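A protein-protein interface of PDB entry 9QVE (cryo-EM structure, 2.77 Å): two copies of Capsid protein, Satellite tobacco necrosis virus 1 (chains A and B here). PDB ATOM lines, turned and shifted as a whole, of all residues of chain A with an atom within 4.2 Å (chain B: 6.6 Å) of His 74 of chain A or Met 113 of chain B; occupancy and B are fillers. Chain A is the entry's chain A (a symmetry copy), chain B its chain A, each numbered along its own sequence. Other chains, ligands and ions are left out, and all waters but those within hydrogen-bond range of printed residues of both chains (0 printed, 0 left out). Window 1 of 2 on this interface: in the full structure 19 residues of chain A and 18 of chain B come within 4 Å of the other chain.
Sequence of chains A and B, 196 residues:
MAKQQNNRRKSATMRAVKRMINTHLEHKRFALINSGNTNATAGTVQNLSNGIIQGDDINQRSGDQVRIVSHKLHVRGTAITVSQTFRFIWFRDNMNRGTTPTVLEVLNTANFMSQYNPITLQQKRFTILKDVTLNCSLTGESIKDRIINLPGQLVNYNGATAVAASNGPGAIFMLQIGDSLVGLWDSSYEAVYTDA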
ATOM      1  N   LEU A  73       4.136 -12.521   7.760  1.00  0.00           N
ATOM      2  CA  LEU A  73       4.322 -11.492   8.772  1.00  0.00           C
ATOM      3  C   LEU A  73       5.069 -12.088   9.952  1.00  0.00           C
ATOM      4  O   LEU A  73       4.726 -13.175  10.427  1.00  0.00           O
ATOM      5  CB  LEU A  73       2.985 -10.912   9.238  1.00  0.00           C
ATOM      6  CG  LEU A  73       3.096  -9.815  10.295  1.00  0.00           C
ATOM      7  CD1 LEU A  73       3.784  -8.600   9.717  1.00  0.00           C
ATOM      8  CD2 LEU A  73       1.736  -9.447  10.853  1.00  0.00           C
ATOM      9  N   HIS A  74       6.084 -11.371  10.422  1.00  0.00           N
ATOM     10  CA  HIS A  74       6.887 -11.783  11.561  1.00  0.00           C
ATOM     11  C   HIS A  74       6.971 -10.618  12.530  1.00  0.00           C
ATOM     12  O   HIS A  74       7.309  -9.501  12.127  1.00  0.00           O
ATOM     13  CB  HIS A  74       8.282 -12.223  11.110  1.00  0.00           C
ATOM     14  CG  HIS A  74       9.144 -12.745  12.214  1.00  0.00           C
ATOM     15  ND1 HIS A  74       8.687 -12.921  13.503  1.00  0.00           N
ATOM     16  CD2 HIS A  74      10.441 -13.133  12.221  1.00  0.00           C
ATOM     17  CE1 HIS A  74       9.666 -13.393  14.254  1.00  0.00           C
ATOM     18  NE2 HIS A  74      10.741 -13.530  13.500  1.00  0.00           N
ATOM     19  N   VAL A  75       6.655 -10.875  13.797  1.00  0.00           N
ATOM     20  CA  VAL A  75       6.671  -9.855  14.835  1.00  0.00           C
ATOM     21  C   VAL A  75       7.434 -10.390  16.037  1.00  0.00           C
ATOM     22  O   VAL A  75       7.564 -11.601  16.234  1.00  0.00           O
ATOM     23  CB  VAL A  75       5.249  -9.418  15.249  1.00  0.00           C
ATOM     24  CG1 VAL A  75       4.550  -8.747  14.096  1.00  0.00           C
ATOM     25  CG2 VAL A  75       4.443 -10.603  15.722  1.00  0.00           C
ATOM     26  N   ARG A  76       7.943  -9.465  16.845  1.00  0.00           N
ATOM     27  CA  ARG A  76       8.746  -9.824  18.009  1.00  0.00           C
ATOM     28  C   ARG A  76       8.738  -8.654  18.974  1.00  0.00           C
ATOM     29  O   ARG A  76       9.138  -7.546  18.603  1.00  0.00           O
ATOM     30  CB  ARG A  76      10.172 -10.177  17.594  1.00  0.00           C
ATOM     31  CG  ARG A  76      11.099 -10.517  18.742  1.00  0.00           C
ATOM     32  CD  ARG A  76      12.421 -11.033  18.227  1.00  0.00           C
ATOM     33  NE  ARG A  76      13.411 -11.193  19.285  1.00  0.00           N
ATOM     34  CZ  ARG A  76      14.167 -10.214  19.758  1.00  0.00           C
ATOM     35  NH1 ARG A  76      14.044  -8.972  19.325  1.00  0.00           N
ATOM     36  NH2 ARG A  76      15.073 -10.489  20.690  1.00  0.00           N
ATOM     37  N   ASP A 145       7.729 -13.976  20.181  1.00  0.00           N
ATOM     38  CA  ASP A 145       7.622 -13.749  18.748  1.00  0.00           C
ATOM     39  C   ASP A 145       6.592 -14.693  18.148  1.00  0.00           C
ATOM     40  O   ASP A 145       6.181 -15.676  18.768  1.00  0.00           O
ATOM     41  CB  ASP A 145       8.970 -13.940  18.045  1.00  0.00           C
ATOM     42  CG  ASP A 145       9.521 -15.341  18.213  1.00  0.00           C
ATOM     43  OD1 ASP A 145       9.415 -15.894  19.327  1.00  0.00           O
ATOM     44  OD2 ASP A 145      10.058 -15.889  17.229  1.00  0.00           O
ATOM     45  N   ARG A 146       6.177 -14.377  16.925  1.00  0.00           N
ATOM     46  CA  ARG A 146       5.209 -15.193  16.210  1.00  0.00           C
ATOM     47  C   ARG A 146       5.351 -14.936  14.717  1.00  0.00           C
ATOM     48  O   ARG A 146       5.689 -13.827  14.294  1.00  0.00           O
ATOM     49  CB  ARG A 146       3.783 -14.895  16.677  1.00  0.00           C
ATOM     50  CG  ARG A 146       2.752 -15.895  16.201  1.00  0.00           C
ATOM     51  CD  ARG A 146       1.561 -15.920  17.135  1.00  0.00           C
ATOM     52  NE  ARG A 146       0.511 -16.816  16.672  1.00  0.00           N
ATOM     53  CZ  ARG A 146      -0.581 -17.102  17.367  1.00  0.00           C
ATOM     54  NH1 ARG A 146      -0.791 -16.583  18.565  1.00  0.00           N
ATOM     55  NH2 ARG A 146      -1.482 -17.930  16.849  1.00  0.00           N
ATOM     56  N   ILE A 147       5.088 -15.973  13.926  1.00  0.00           N
ATOM     57  CA  ILE A 147       5.192 -15.922  12.474  1.00  0.00           C
ATOM     58  C   ILE A 147       3.860 -16.355  11.880  1.00  0.00           C
ATOM     59  O   ILE A 147       3.285 -17.363  12.303  1.00  0.00           O
ATOM     60  CB  ILE A 147       6.336 -16.812  11.950  1.00  0.00           C
ATOM     61  CG1 ILE A 147       7.684 -16.338  12.496  1.00  0.00           C
ATOM     62  CG2 ILE A 147       6.359 -16.802  10.437  1.00  0.00           C
ATOM     63  CD1 ILE A 147       8.108 -17.025  13.776  1.00  0.00           C
ATOM     64  N   ASP A 186       9.741  -5.354  16.987  1.00  0.00           N
ATOM     65  CA  ASP A 186      10.347  -5.464  15.670  1.00  0.00           C
ATOM     66  C   ASP A 186       9.456  -6.327  14.792  1.00  0.00           C
ATOM     67  O   ASP A 186       8.663  -7.134  15.282  1.00  0.00           O
ATOM     68  CB  ASP A 186      11.752  -6.067  15.748  1.00  0.00           C
ATOM     69  CG  ASP A 186      12.549  -5.538  16.925  1.00  0.00           C
ATOM     70  OD1 ASP A 186      12.387  -4.351  17.269  1.00  0.00           O
ATOM     71  OD2 ASP A 186      13.334  -6.315  17.507  1.00  0.00           O
ATOM     72  N   SER A 187       9.592  -6.154  13.478  1.00  0.00           N
ATOM     73  CA  SER A 187       8.739  -6.874  12.546  1.00  0.00           C
ATOM     74  C   SER A 187       9.433  -7.018  11.202  1.00  0.00           C
ATOM     75  O   SER A 187      10.407  -6.327  10.900  1.00  0.00           O
ATOM     76  CB  SER A 187       7.395  -6.168  12.357  1.00  0.00           C
ATOM     77  OG  SER A 187       7.553  -4.979  11.609  1.00  0.00           O
ATOM     78  N   SER A 188       8.906  -7.938  10.399  1.00  0.00           N
ATOM     79  CA  SER A 188       9.350  -8.137   9.029  1.00  0.00           C
ATOM     80  C   SER A 188       8.157  -8.601   8.207  1.00  0.00           C
ATOM     81  O   SER A 188       7.192  -9.155   8.738  1.00  0.00           O
ATOM     82  CB  SER A 188      10.494  -9.153   8.944  1.00  0.00           C
ATOM     83  OG  SER A 188      11.587  -8.754   9.746  1.00  0.00           O
ATOM     84  N   ARG B  87      18.289 -17.862  16.136  1.00  0.00           N
ATOM     85  CA  ARG B  87      17.592 -18.253  14.920  1.00  0.00           C
ATOM     86  C   ARG B  87      18.436 -19.272  14.173  1.00  0.00           C
ATOM     87  O   ARG B  87      19.632 -19.055  13.959  1.00  0.00           O
ATOM     88  CB  ARG B  87      17.304 -17.051  14.019  1.00  0.00           C
ATOM     89  CG  ARG B  87      16.412 -17.392  12.841  1.00  0.00           C
ATOM     90  CD  ARG B  87      16.126 -16.196  11.964  1.00  0.00           C
ATOM     91  NE  ARG B  87      15.400 -16.581  10.759  1.00  0.00           N
ATOM     92  CZ  ARG B  87      15.004 -15.735   9.818  1.00  0.00           C
ATOM     93  NH1 ARG B  87      15.234 -14.438   9.915  1.00  0.00           N
ATOM     94  NH2 ARG B  87      14.361 -16.203   8.754  1.00  0.00           N
ATOM     95  N   LEU B 107      19.485 -14.313   3.218  1.00  0.00           N
ATOM     96  CA  LEU B 107      18.637 -13.319   3.850  1.00  0.00           C
ATOM     97  C   LEU B 107      18.803 -11.982   3.146  1.00  0.00           C
ATOM     98  O   LEU B 107      19.882 -11.649   2.653  1.00  0.00           O
ATOM     99  CB  LEU B 107      18.969 -13.167   5.338  1.00  0.00           C
ATOM    100  CG  LEU B 107      18.815 -14.416   6.208  1.00  0.00           C
ATOM    101  CD1 LEU B 107      19.209 -14.117   7.636  1.00  0.00           C
ATOM    102  CD2 LEU B 107      17.400 -14.949   6.160  1.00  0.00           C
ATOM    103  N   THR B 109      18.755  -9.043   4.514  1.00  0.00           N
ATOM    104  CA  THR B 109      19.710  -8.287   5.310  1.00  0.00           C
ATOM    105  C   THR B 109      20.256  -9.186   6.408  1.00  0.00           C
ATOM    106  O   THR B 109      19.627 -10.168   6.806  1.00  0.00           O
ATOM    107  CB  THR B 109      19.079  -7.031   5.923  1.00  0.00           C
ATOM    108  OG1 THR B 109      17.888  -7.388   6.634  1.00  0.00           O
ATOM    109  CG2 THR B 109      18.741  -6.023   4.845  1.00  0.00           C
ATOM    110  N   ALA B 110      21.446  -8.834   6.896  1.00  0.00           N
ATOM    111  CA  ALA B 110      22.118  -9.607   7.940  1.00  0.00           C
ATOM    112  C   ALA B 110      21.524  -9.289   9.315  1.00  0.00           C
ATOM    113  O   ALA B 110      22.182  -8.764  10.212  1.00  0.00           O
ATOM    114  CB  ALA B 110      23.615  -9.335   7.910  1.00  0.00           C
ATOM    115  N   ASN B 111      20.245  -9.624   9.463  1.00  0.00           N
ATOM    116  CA  ASN B 111      19.522  -9.422  10.708  1.00  0.00           C
ATOM    117  C   ASN B 111      18.675 -10.652  10.996  1.00  0.00           C
ATOM    118  O   ASN B 111      18.097 -11.244  10.081  1.00  0.00           O
ATOM    119  CB  ASN B 111      18.635  -8.176  10.643  1.00  0.00           C
ATOM    120  CG  ASN B 111      17.926  -7.898  11.947  1.00  0.00           C
ATOM    121  OD1 ASN B 111      16.900  -8.501  12.250  1.00  0.00           O
ATOM    122  ND2 ASN B 111      18.470  -6.978  12.726  1.00  0.00           N
ATOM    123  N   PHE B 112      18.606 -11.030  12.273  1.00  0.00           N
ATOM    124  CA  PHE B 112      17.822 -12.195  12.664  1.00  0.00           C
ATOM    125  C   PHE B 112      16.349 -12.047  12.314  1.00  0.00           C
ATOM    126  O   PHE B 112      15.652 -13.059  12.180  1.00  0.00           O
ATOM    127  CB  PHE B 112      17.986 -12.456  14.164  1.00  0.00           C
ATOM    128  CG  PHE B 112      17.439 -11.368  15.039  1.00  0.00           C
ATOM    129  CD1 PHE B 112      18.115 -10.171  15.185  1.00  0.00           C
ATOM    130  CD2 PHE B 112      16.260 -11.550  15.734  1.00  0.00           C
ATOM    131  CE1 PHE B 112      17.615  -9.174  15.989  1.00  0.00           C
ATOM    132  CE2 PHE B 112      15.760 -10.556  16.541  1.00  0.00           C
ATOM    133  CZ  PHE B 112      16.439  -9.367  16.670  1.00  0.00           C
ATOM    134  N   MET B 113      15.858 -10.821  12.159  1.00  0.00           N
ATOM    135  CA  MET B 113      14.484 -10.579  11.742  1.00  0.00           C
ATOM    136  C   MET B 113      14.325 -10.571  10.230  1.00  0.00           C
ATOM    137  O   MET B 113      13.205 -10.399   9.740  1.00  0.00           O
ATOM    138  CB  MET B 113      13.988  -9.246  12.307  1.00  0.00           C
ATOM    139  CG  MET B 113      14.020  -9.153  13.816  1.00  0.00           C
ATOM    140  SD  MET B 113      12.956 -10.362  14.617  1.00  0.00           S
ATOM    141  CE  MET B 113      11.354  -9.789  14.073  1.00  0.00           C
ATOM    142  N   SER B 114      15.411 -10.751   9.487  1.00  0.00           N
ATOM    143  CA  SER B 114      15.360 -10.632   8.040  1.00  0.00           C
ATOM    144  C   SER B 114      14.573 -11.777   7.421  1.00  0.00           C
ATOM    145  O   SER B 114      14.506 -12.884   7.960  1.00  0.00           O
ATOM    146  CB  SER B 114      16.770 -10.611   7.459  1.00  0.00           C
ATOM    147  OG  SER B 114      16.732 -10.547   6.048  1.00  0.00           O
ATOM    148  N   GLN B 115      13.968 -11.492   6.274  1.00  0.00           N
ATOM    149  CA  GLN B 115      13.292 -12.498   5.476  1.00  0.00           C
ATOM    150  C   GLN B 115      14.258 -13.087   4.452  1.00  0.00           C
ATOM    151  O   GLN B 115      15.352 -12.572   4.220  1.00  0.00           O
ATOM    152  CB  GLN B 115      12.075 -11.893   4.782  1.00  0.00           C
ATOM    153  CG  GLN B 115      10.953 -11.515   5.721  1.00  0.00           C
ATOM    154  CD  GLN B 115      10.220 -12.723   6.259  1.00  0.00           C
ATOM    155  OE1 GLN B 115      10.569 -13.863   5.956  1.00  0.00           O
ATOM    156  NE2 GLN B 115       9.195 -12.480   7.061  1.00  0.00           N
ATOM    157  N   THR B 133      13.415 -20.455  15.641  1.00  0.00           N
ATOM    158  CA  THR B 133      13.795 -19.281  16.416  1.00  0.00           C
ATOM    159  C   THR B 133      13.557 -19.585  17.885  1.00  0.00           C
ATOM    160  O   THR B 133      12.435 -19.923  18.278  1.00  0.00           O
ATOM    161  CB  THR B 133      12.996 -18.050  15.982  1.00  0.00           C
ATOM    162  OG1 THR B 133      12.960 -17.978  14.551  1.00  0.00           O
ATOM    163  CG2 THR B 133      13.630 -16.783  16.528  1.00  0.00           C
ATOM    164  N   ILE B 177      21.961 -17.096  13.434  1.00  0.00           N
ATOM    165  CA  ILE B 177      22.008 -15.643  13.523  1.00  0.00           C
ATOM    166  C   ILE B 177      21.133 -15.215  14.691  1.00  0.00           C
ATOM    167  O   ILE B 177      20.056 -15.775  14.913  1.00  0.00           O
ATOM    168  CB  ILE B 177      21.558 -14.996  12.193  1.00  0.00           C
ATOM    169  CG1 ILE B 177      21.810 -13.491  12.217  1.00  0.00           C
ATOM    170  CG2 ILE B 177      20.093 -15.299  11.923  1.00  0.00           C
ATOM    171  CD1 ILE B 177      21.809 -12.869  10.853  1.00  0.00           C
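The backbone carbonyl oxygen (O) of Met 113 of chain B sits close to the side-chain hydroxyl (OG) of Ser 188 of chain A.
The side-chain amide oxygen (OD1) of Asn 111 of chain B lies within hydrogen-bond range of the backbone NH (N) of Met 113 of chain B, 2.5 Å away. The backbone NH of Ser 188 of chain A is in hydrogen-bond range of the backbone carbonyl oxygen of His 74 of chain A. The guanidinium group (NH1) of Arg 87 of chain B lies within hydrogen-bond range of the backbone carbonyl oxygen (O) of Phe 112 of chain B (2.7 Å). OD2 of Asp 186 of chain A is in salt-bridge range of NH1 of Arg 76 of chain A (3.3 Å). The backbone carbonyl oxygen (O) of Arg 146 of chain A sits at hydrogen-bond distance from a ring nitrogen (ND1) of His 74 of chain A (3.2 Å).
Among the printed residues, pairs that only touch across the chains: His 74 of chain A with Met 113 of chain B, Arg 76 of chain A with Phe 112 of chain B, Arg 76 of chain A with Met 113 of chain B, Asp 145 of chain A with Thr 133 of chain B and Asp 186 of chain A with Met 113 of chain B.
His 74 of chain A touches just one residue of chain B: Met 113 (3.8 Å). Of chain A, only His 74, Arg 76, Asp 186 and Ser 188 come within 4 Å of Met 113 of chain B. Printed residues of chain B within 4 Å of Arg 76 of chain A: Phe 112 (3.6 Å) and Met 113 (3.7 Å). Of the printed residues of chain B, Asp 186 of chain A touches Met 113 (3.97 Å). Printed residues of chain B within 4 Å of Ser 188 of chain A: Met 113 (2.3 Å). Asn 111 of chain B touches none of the printed residues of chain A. The nearest residue of chain A that does not touch Met 113 of chain B is Ser 187 of chain A (4.1 Å). The nearest printed residue of chain A that does not touch Phe 112 of chain B is Asp 186 of chain A (4.4 Å).
Printed residues of chain B that touch a printed residue of chain A: Phe 112, Met 113 and Thr 133. Hydrophobic or aromatic side chains of chain A within 4 Å of the printed part of chain B: His 74. Among the printed residues, 6 pairs touch across the chains.
No position is printed for both chains. Of the 6 pairs that touch across the chains among the printed residues, none has its exchanged pair printed and touching as well.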
